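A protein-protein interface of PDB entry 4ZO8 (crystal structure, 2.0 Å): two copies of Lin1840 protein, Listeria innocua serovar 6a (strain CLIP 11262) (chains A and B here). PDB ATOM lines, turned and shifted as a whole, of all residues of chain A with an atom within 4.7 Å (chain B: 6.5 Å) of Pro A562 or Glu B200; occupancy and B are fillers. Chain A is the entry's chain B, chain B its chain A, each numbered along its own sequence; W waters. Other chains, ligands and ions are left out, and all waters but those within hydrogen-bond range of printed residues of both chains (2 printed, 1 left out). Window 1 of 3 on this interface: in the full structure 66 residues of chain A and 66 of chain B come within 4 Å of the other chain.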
ATOM      1  N   ARG A 143     -10.659  27.125  20.302  1.00  0.00           N
ATOM      2  CA  ARG A 143     -10.841  26.651  18.949  1.00  0.00           C
ATOM      3  C   ARG A 143     -12.034  27.272  18.194  1.00  0.00           C
ATOM      4  O   ARG A 143     -12.288  26.900  17.052  1.00  0.00           O
ATOM      5  CB  ARG A 143     -11.032  25.131  18.921  1.00  0.00           C
ATOM      6  CG  ARG A 143      -9.920  24.377  19.578  1.00  0.00           C
ATOM      7  CD  ARG A 143     -10.152  22.895  19.541  1.00  0.00           C
ATOM      8  NE  ARG A 143      -8.925  22.188  19.781  1.00  0.00           N
ATOM      9  CZ  ARG A 143      -8.848  20.891  20.040  1.00  0.00           C
ATOM     10  NH1 ARG A 143      -9.931  20.155  20.078  1.00  0.00           N
ATOM     11  NH2 ARG A 143      -7.678  20.331  20.270  1.00  0.00           N
ATOM     12  N   GLN A 560     -16.999  26.255   9.059  1.00  0.00           N
ATOM     13  CA  GLN A 560     -15.801  25.430   9.168  1.00  0.00           C
ATOM     14  C   GLN A 560     -15.415  25.206  10.628  1.00  0.00           C
ATOM     15  O   GLN A 560     -14.607  24.345  10.902  1.00  0.00           O
ATOM     16  CB  GLN A 560     -14.632  26.058   8.430  1.00  0.00           C
ATOM     17  CG  GLN A 560     -13.497  25.096   8.156  1.00  0.00           C
ATOM     18  CD  GLN A 560     -12.386  25.731   7.346  1.00  0.00           C
ATOM     19  OE1 GLN A 560     -11.888  26.828   7.646  1.00  0.00           O
ATOM     20  NE2 GLN A 560     -11.980  25.034   6.335  1.00  0.00           N
ATOM     21  N   ILE A 561     -15.992  25.966  11.560  1.00  0.00           N
ATOM     22  CA  ILE A 561     -15.554  25.925  12.972  1.00  0.00           C
ATOM     23  C   ILE A 561     -16.014  24.637  13.696  1.00  0.00           C
ATOM     24  O   ILE A 561     -17.155  24.207  13.511  1.00  0.00           O
ATOM     25  CB  ILE A 561     -16.106  27.144  13.741  1.00  0.00           C
ATOM     26  CG1 ILE A 561     -15.486  28.412  13.227  1.00  0.00           C
ATOM     27  CG2 ILE A 561     -15.825  27.041  15.216  1.00  0.00           C
ATOM     28  CD1 ILE A 561     -16.276  29.645  13.534  1.00  0.00           C
ATOM     29  N   PRO A 562     -15.136  24.006  14.491  1.00  0.00           N
ATOM     30  CA  PRO A 562     -13.790  24.341  14.737  1.00  0.00           C
ATOM     31  C   PRO A 562     -12.868  23.796  13.683  1.00  0.00           C
ATOM     32  O   PRO A 562     -12.988  22.658  13.254  1.00  0.00           O
ATOM     33  CB  PRO A 562     -13.519  23.724  16.107  1.00  0.00           C
ATOM     34  CG  PRO A 562     -14.296  22.448  16.074  1.00  0.00           C
ATOM     35  CD  PRO A 562     -15.529  22.797  15.241  1.00  0.00           C
ATOM     36  N   VAL A 563     -11.901  24.627  13.318  1.00  0.00           N
ATOM     37  CA  VAL A 563     -10.798  24.211  12.466  1.00  0.00           C
ATOM     38  C   VAL A 563      -9.505  24.660  13.157  1.00  0.00           C
ATOM     39  O   VAL A 563      -9.454  25.783  13.713  1.00  0.00           O
ATOM     40  CB  VAL A 563     -10.941  24.819  11.053  1.00  0.00           C
ATOM     41  CG1 VAL A 563     -10.930  26.332  11.093  1.00  0.00           C
ATOM     42  CG2 VAL A 563      -9.876  24.298  10.129  1.00  0.00           C
ATOM     43  N   TYR A 564      -8.500  23.789  13.157  1.00  0.00           N
ATOM     44  CA  TYR A 564      -7.288  24.044  13.956  1.00  0.00           C
ATOM     45  C   TYR A 564      -6.156  23.136  13.456  1.00  0.00           C
ATOM     46  O   TYR A 564      -6.450  22.067  12.875  1.00  0.00           O
ATOM     47  CB  TYR A 564      -7.539  23.873  15.472  1.00  0.00           C
ATOM     48  CG  TYR A 564      -8.257  22.591  15.818  1.00  0.00           C
ATOM     49  CD1 TYR A 564      -7.545  21.408  16.044  1.00  0.00           C
ATOM     50  CD2 TYR A 564      -9.662  22.518  15.908  1.00  0.00           C
ATOM     51  CE1 TYR A 564      -8.180  20.201  16.320  1.00  0.00           C
ATOM     52  CE2 TYR A 564     -10.279  21.297  16.170  1.00  0.00           C
ATOM     53  CZ  TYR A 564      -9.513  20.178  16.413  1.00  0.00           C
ATOM     54  OH  TYR A 564     -10.089  18.990  16.685  1.00  0.00           O
ATOM     55  N   ASP B 144     -26.130  18.359  14.307  1.00  0.00           N
ATOM     56  CA  ASP B 144     -25.350  19.158  13.398  1.00  0.00           C
ATOM     57  C   ASP B 144     -25.806  18.926  11.957  1.00  0.00           C
ATOM     58  O   ASP B 144     -25.333  18.017  11.265  1.00  0.00           O
ATOM     59  CB  ASP B 144     -23.862  18.836  13.593  1.00  0.00           C
ATOM     60  CG  ASP B 144     -22.942  19.825  12.899  1.00  0.00           C
ATOM     61  OD1 ASP B 144     -23.426  20.565  12.006  1.00  0.00           O
ATOM     62  OD2 ASP B 144     -21.737  19.902  13.287  1.00  0.00           O
ATOM     63  N   ARG B 146     -24.914  20.366   9.272  1.00  0.00           N
ATOM     64  CA  ARG B 146     -23.863  20.371   8.237  1.00  0.00           C
ATOM     65  C   ARG B 146     -23.605  18.955   7.710  1.00  0.00           C
ATOM     66  O   ARG B 146     -23.334  18.775   6.545  1.00  0.00           O
ATOM     67  CB  ARG B 146     -22.587  21.016   8.750  1.00  0.00           C
ATOM     68  CG  ARG B 146     -22.749  22.522   9.019  1.00  0.00           C
ATOM     69  CD  ARG B 146     -21.531  23.118   9.743  1.00  0.00           C
ATOM     70  NE  ARG B 146     -21.440  22.609  11.107  1.00  0.00           N
ATOM     71  CZ  ARG B 146     -20.682  23.069  12.086  1.00  0.00           C
ATOM     72  NH1 ARG B 146     -19.775  23.994  11.902  1.00  0.00           N
ATOM     73  NH2 ARG B 146     -20.765  22.501  13.267  1.00  0.00           N
ATOM     74  N   TYR B 196     -21.380   8.422  15.731  1.00  0.00           N
ATOM     75  CA  TYR B 196     -20.888   8.892  14.428  1.00  0.00           C
ATOM     76  C   TYR B 196     -21.407  10.296  14.039  1.00  0.00           C
ATOM     77  O   TYR B 196     -20.664  11.117  13.448  1.00  0.00           O
ATOM     78  CB  TYR B 196     -21.280   7.818  13.388  1.00  0.00           C
ATOM     79  CG  TYR B 196     -20.905   8.019  11.956  1.00  0.00           C
ATOM     80  CD1 TYR B 196     -19.737   8.679  11.559  1.00  0.00           C
ATOM     81  CD2 TYR B 196     -21.669   7.472  10.974  1.00  0.00           C
ATOM     82  CE1 TYR B 196     -19.400   8.805  10.190  1.00  0.00           C
ATOM     83  CE2 TYR B 196     -21.335   7.593   9.645  1.00  0.00           C
ATOM     84  CZ  TYR B 196     -20.222   8.265   9.261  1.00  0.00           C
ATOM     85  OH  TYR B 196     -20.013   8.393   7.918  1.00  0.00           O
ATOM     86  N   ALA B 198     -21.794  12.919  15.747  1.00  0.00           N
ATOM     87  CA  ALA B 198     -21.222  14.038  16.482  1.00  0.00           C
ATOM     88  C   ALA B 198     -19.936  14.515  15.784  1.00  0.00           C
ATOM     89  O   ALA B 198     -19.155  15.282  16.335  1.00  0.00           O
ATOM     90  CB  ALA B 198     -20.998  13.667  17.929  1.00  0.00           C
ATOM     91  N   ALA B 199     -19.736  14.067  14.537  1.00  0.00           N
ATOM     92  CA  ALA B 199     -18.572  14.481  13.731  1.00  0.00           C
ATOM     93  C   ALA B 199     -18.286  15.959  13.837  1.00  0.00           C
ATOM     94  O   ALA B 199     -19.185  16.812  13.611  1.00  0.00           O
ATOM     95  CB  ALA B 199     -18.821  14.146  12.268  1.00  0.00           C
ATOM     96  N   GLU B 200     -17.037  16.276  14.181  1.00  0.00           N
ATOM     97  CA  GLU B 200     -16.699  17.646  14.482  1.00  0.00           C
ATOM     98  C   GLU B 200     -16.901  18.505  13.223  1.00  0.00           C
ATOM     99  O   GLU B 200     -16.555  18.082  12.099  1.00  0.00           O
ATOM    100  CB  GLU B 200     -15.255  17.767  14.959  1.00  0.00           C
ATOM    101  CG  GLU B 200     -14.882  19.084  15.606  1.00  0.00           C
ATOM    102  CD  GLU B 200     -13.683  18.923  16.566  1.00  0.00           C
ATOM    103  OE1 GLU B 200     -12.575  19.093  16.041  1.00  0.00           O
ATOM    104  OE2 GLU B 200     -13.850  18.604  17.813  1.00  0.00           O
ATOM    105  N   ALA B 201     -17.486  19.692  13.447  1.00  0.00           N
ATOM    106  CA  ALA B 201     -17.781  20.669  12.372  1.00  0.00           C
ATOM    107  C   ALA B 201     -18.671  20.137  11.262  1.00  0.00           C
ATOM    108  O   ALA B 201     -18.625  20.673  10.149  1.00  0.00           O
ATOM    109  CB  ALA B 201     -16.485  21.197  11.775  1.00  0.00           C
ATOM    110  N   GLY B 202     -19.459  19.097  11.530  1.00  0.00           N
ATOM    111  CA  GLY B 202     -20.280  18.402  10.469  1.00  0.00           C
ATOM    112  C   GLY B 202     -19.516  17.773   9.315  1.00  0.00           C
ATOM    113  O   GLY B 202     -20.067  17.513   8.258  1.00  0.00           O
ATOM    114  N   LEU B 203     -18.219  17.626   9.494  1.00  0.00           N
ATOM    115  CA  LEU B 203     -17.317  17.128   8.429  1.00  0.00           C
ATOM    116  C   LEU B 203     -17.296  15.588   8.334  1.00  0.00           C
ATOM    117  O   LEU B 203     -17.065  14.922   9.302  1.00  0.00           O
ATOM    118  CB  LEU B 203     -15.892  17.666   8.644  1.00  0.00           C
ATOM    119  CG  LEU B 203     -14.841  17.191   7.656  1.00  0.00           C
ATOM    120  CD1 LEU B 203     -15.264  17.569   6.250  1.00  0.00           C
ATOM    121  CD2 LEU B 203     -13.435  17.780   7.974  1.00  0.00           C
ATOM    122  N   GLU B 204     -17.505  15.028   7.151  1.00  0.00           N
ATOM    123  CA  GLU B 204     -17.614  13.576   7.049  1.00  0.00           C
ATOM    124  C   GLU B 204     -16.364  12.849   7.604  1.00  0.00           C
ATOM    125  O   GLU B 204     -15.200  13.262   7.384  1.00  0.00           O
ATOM    126  CB  GLU B 204     -17.930  13.125   5.628  1.00  0.00           C
ATOM    127  CG  GLU B 204     -18.418  11.723   5.559  1.00  0.00           C
ATOM    128  CD  GLU B 204     -19.689  11.540   6.372  1.00  0.00           C
ATOM    129  OE1 GLU B 204     -20.831  11.849   5.873  1.00  0.00           O
ATOM    130  OE2 GLU B 204     -19.541  11.040   7.495  1.00  0.00           O
ATOM    131  N   ASN B 206     -15.110  12.818  10.473  1.00  0.00           N
ATOM    132  CA  ASN B 206     -14.245  13.624  11.327  1.00  0.00           C
ATOM    133  C   ASN B 206     -14.368  13.216  12.816  1.00  0.00           C
ATOM    134  O   ASN B 206     -15.298  12.490  13.229  1.00  0.00           O
ATOM    135  CB  ASN B 206     -14.500  15.106  11.136  1.00  0.00           C
ATOM    136  CG  ASN B 206     -13.338  15.985  11.585  1.00  0.00           C
ATOM    137  OD1 ASN B 206     -12.161  15.563  11.680  1.00  0.00           O
ATOM    138  ND2 ASN B 206     -13.656  17.244  11.807  1.00  0.00           N
ATOM    139  N   THR B 207     -13.357  13.635  13.565  1.00  0.00           N
ATOM    140  CA  THR B 207     -13.237  13.419  15.001  1.00  0.00           C
ATOM    141  C   THR B 207     -14.561  13.553  15.738  1.00  0.00           C
ATOM    142  O   THR B 207     -15.331  14.436  15.472  1.00  0.00           O
ATOM    143  CB  THR B 207     -12.249  14.419  15.557  1.00  0.00           C
ATOM    144  OG1 THR B 207     -10.984  14.179  14.888  1.00  0.00           O
ATOM    145  CG2 THR B 207     -12.112  14.268  17.071  1.00  0.00           C
ATOM    146  N   VAL B 208     -14.779  12.647  16.679  1.00  0.00           N
ATOM    147  CA  VAL B 208     -15.886  12.714  17.628  1.00  0.00           C
ATOM    148  C   VAL B 208     -15.270  12.697  19.005  1.00  0.00           C
ATOM    149  O   VAL B 208     -14.343  11.918  19.271  1.00  0.00           O
ATOM    150  CB  VAL B 208     -16.825  11.503  17.433  1.00  0.00           C
ATOM    151  CG1 VAL B 208     -17.791  11.358  18.619  1.00  0.00           C
ATOM    152  CG2 VAL B 208     -17.603  11.617  16.094  1.00  0.00           C
ATOM    153  N   ASN B 209     -15.729  13.560  19.884  1.00  0.00           N
ATOM    154  CA  ASN B 209     -15.282  13.529  21.282  1.00  0.00           C
ATOM    155  C   ASN B 209     -16.370  14.056  22.203  1.00  0.00           C
ATOM    156  O   ASN B 209     -16.928  15.101  21.924  1.00  0.00           O
ATOM    157  CB  ASN B 209     -14.022  14.339  21.511  1.00  0.00           C
ATOM    158  CG  ASN B 209     -13.467  14.123  22.899  1.00  0.00           C
ATOM    159  OD1 ASN B 209     -13.751  14.889  23.828  1.00  0.00           O
ATOM    160  ND2 ASN B 209     -12.723  13.052  23.068  1.00  0.00           N
HETATM  161  O   HOH W   1     -12.600  20.308  11.758  1.00  0.00           O
HETATM  162  O   HOH W   2      -9.678  16.428  15.011  1.00  0.00           O
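Among the printed residues, merely in contact across the chains: Pro A562 with Glu B200, Ile A561 with Ala B201, Gln A560 with Ala B201 and Pro A562 with Ala B201.
The backbone NH (N) of Glu B200 is in hydrogen-bond range of the backbone carbonyl oxygen (O) of Thr B207, at 2.8 Å. OD2 of Asp B144 lies within salt-bridge range of NH2 of Arg B146, 2.8 Å away. The backbone carbonyl oxygen (O) of Glu B200 is in hydrogen-bond range of the side-chain amide nitrogen (ND2) of Asn B206 (3.0 Å).
Of the printed residues of chain B, Gln A560 touches Ala B201 (3.8 Å). Of chain B, only Glu B200 and Ala B201 come within 4 Å of Pro A562. Of the printed residues of chain B, Tyr A564 touches Glu B200 (2.6 Å). Printed residues of chain A within 4 Å of Arg B146: Ile A561. Glu B200 touches just these residues of chain A: Pro A562 and Tyr A564. Of the printed residues of chain A, Ala B201 touches Gln A560, Ile A561 and Pro A562. The nearest residue of chain B that does not touch Pro A562 is Arg B146 (5.3 Å).
Water W2 bridges the side-chain hydroxyl (OG1) of Thr B207 (2.6 Å) and the side-chain hydroxyl (OH) of Tyr A564 (3.1 Å). Water W1 bridges the backbone carbonyl oxygen of Pro A562 and the side-chain amide nitrogen of Asn B206.
No position is printed for both chains. Of the 6 pairs that touch across the chains among the printed residues, none has its exchanged pair printed and touching as well.
OE1 of Glu B200 lies within hydrogen-bond range of OH of Tyr A564 (2.6 Å). The guanidinium group (NH1) of Arg B146 is in hydrogen-bond range of the backbone carbonyl oxygen (O) of Ile A561 (3.1 Å).
Of the 14 printed residues of chain B, 3 touch a printed residue of chain A. Printed residues of chain B that touch a printed residue of chain A: Arg B146, Glu B200 and Ala B201. Hydrophobic or aromatic side chains of chain B within 4 Å of the printed part of chain A: Ala B201. Of the 6 printed residues of chain A, 4 touch a printed residue of chain B. Hydrophobic or aromatic side chains of chain A that line the printed part of chain B: Pro A562 and Tyr A564. Among the printed residues, 6 pairs touch across the chains.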
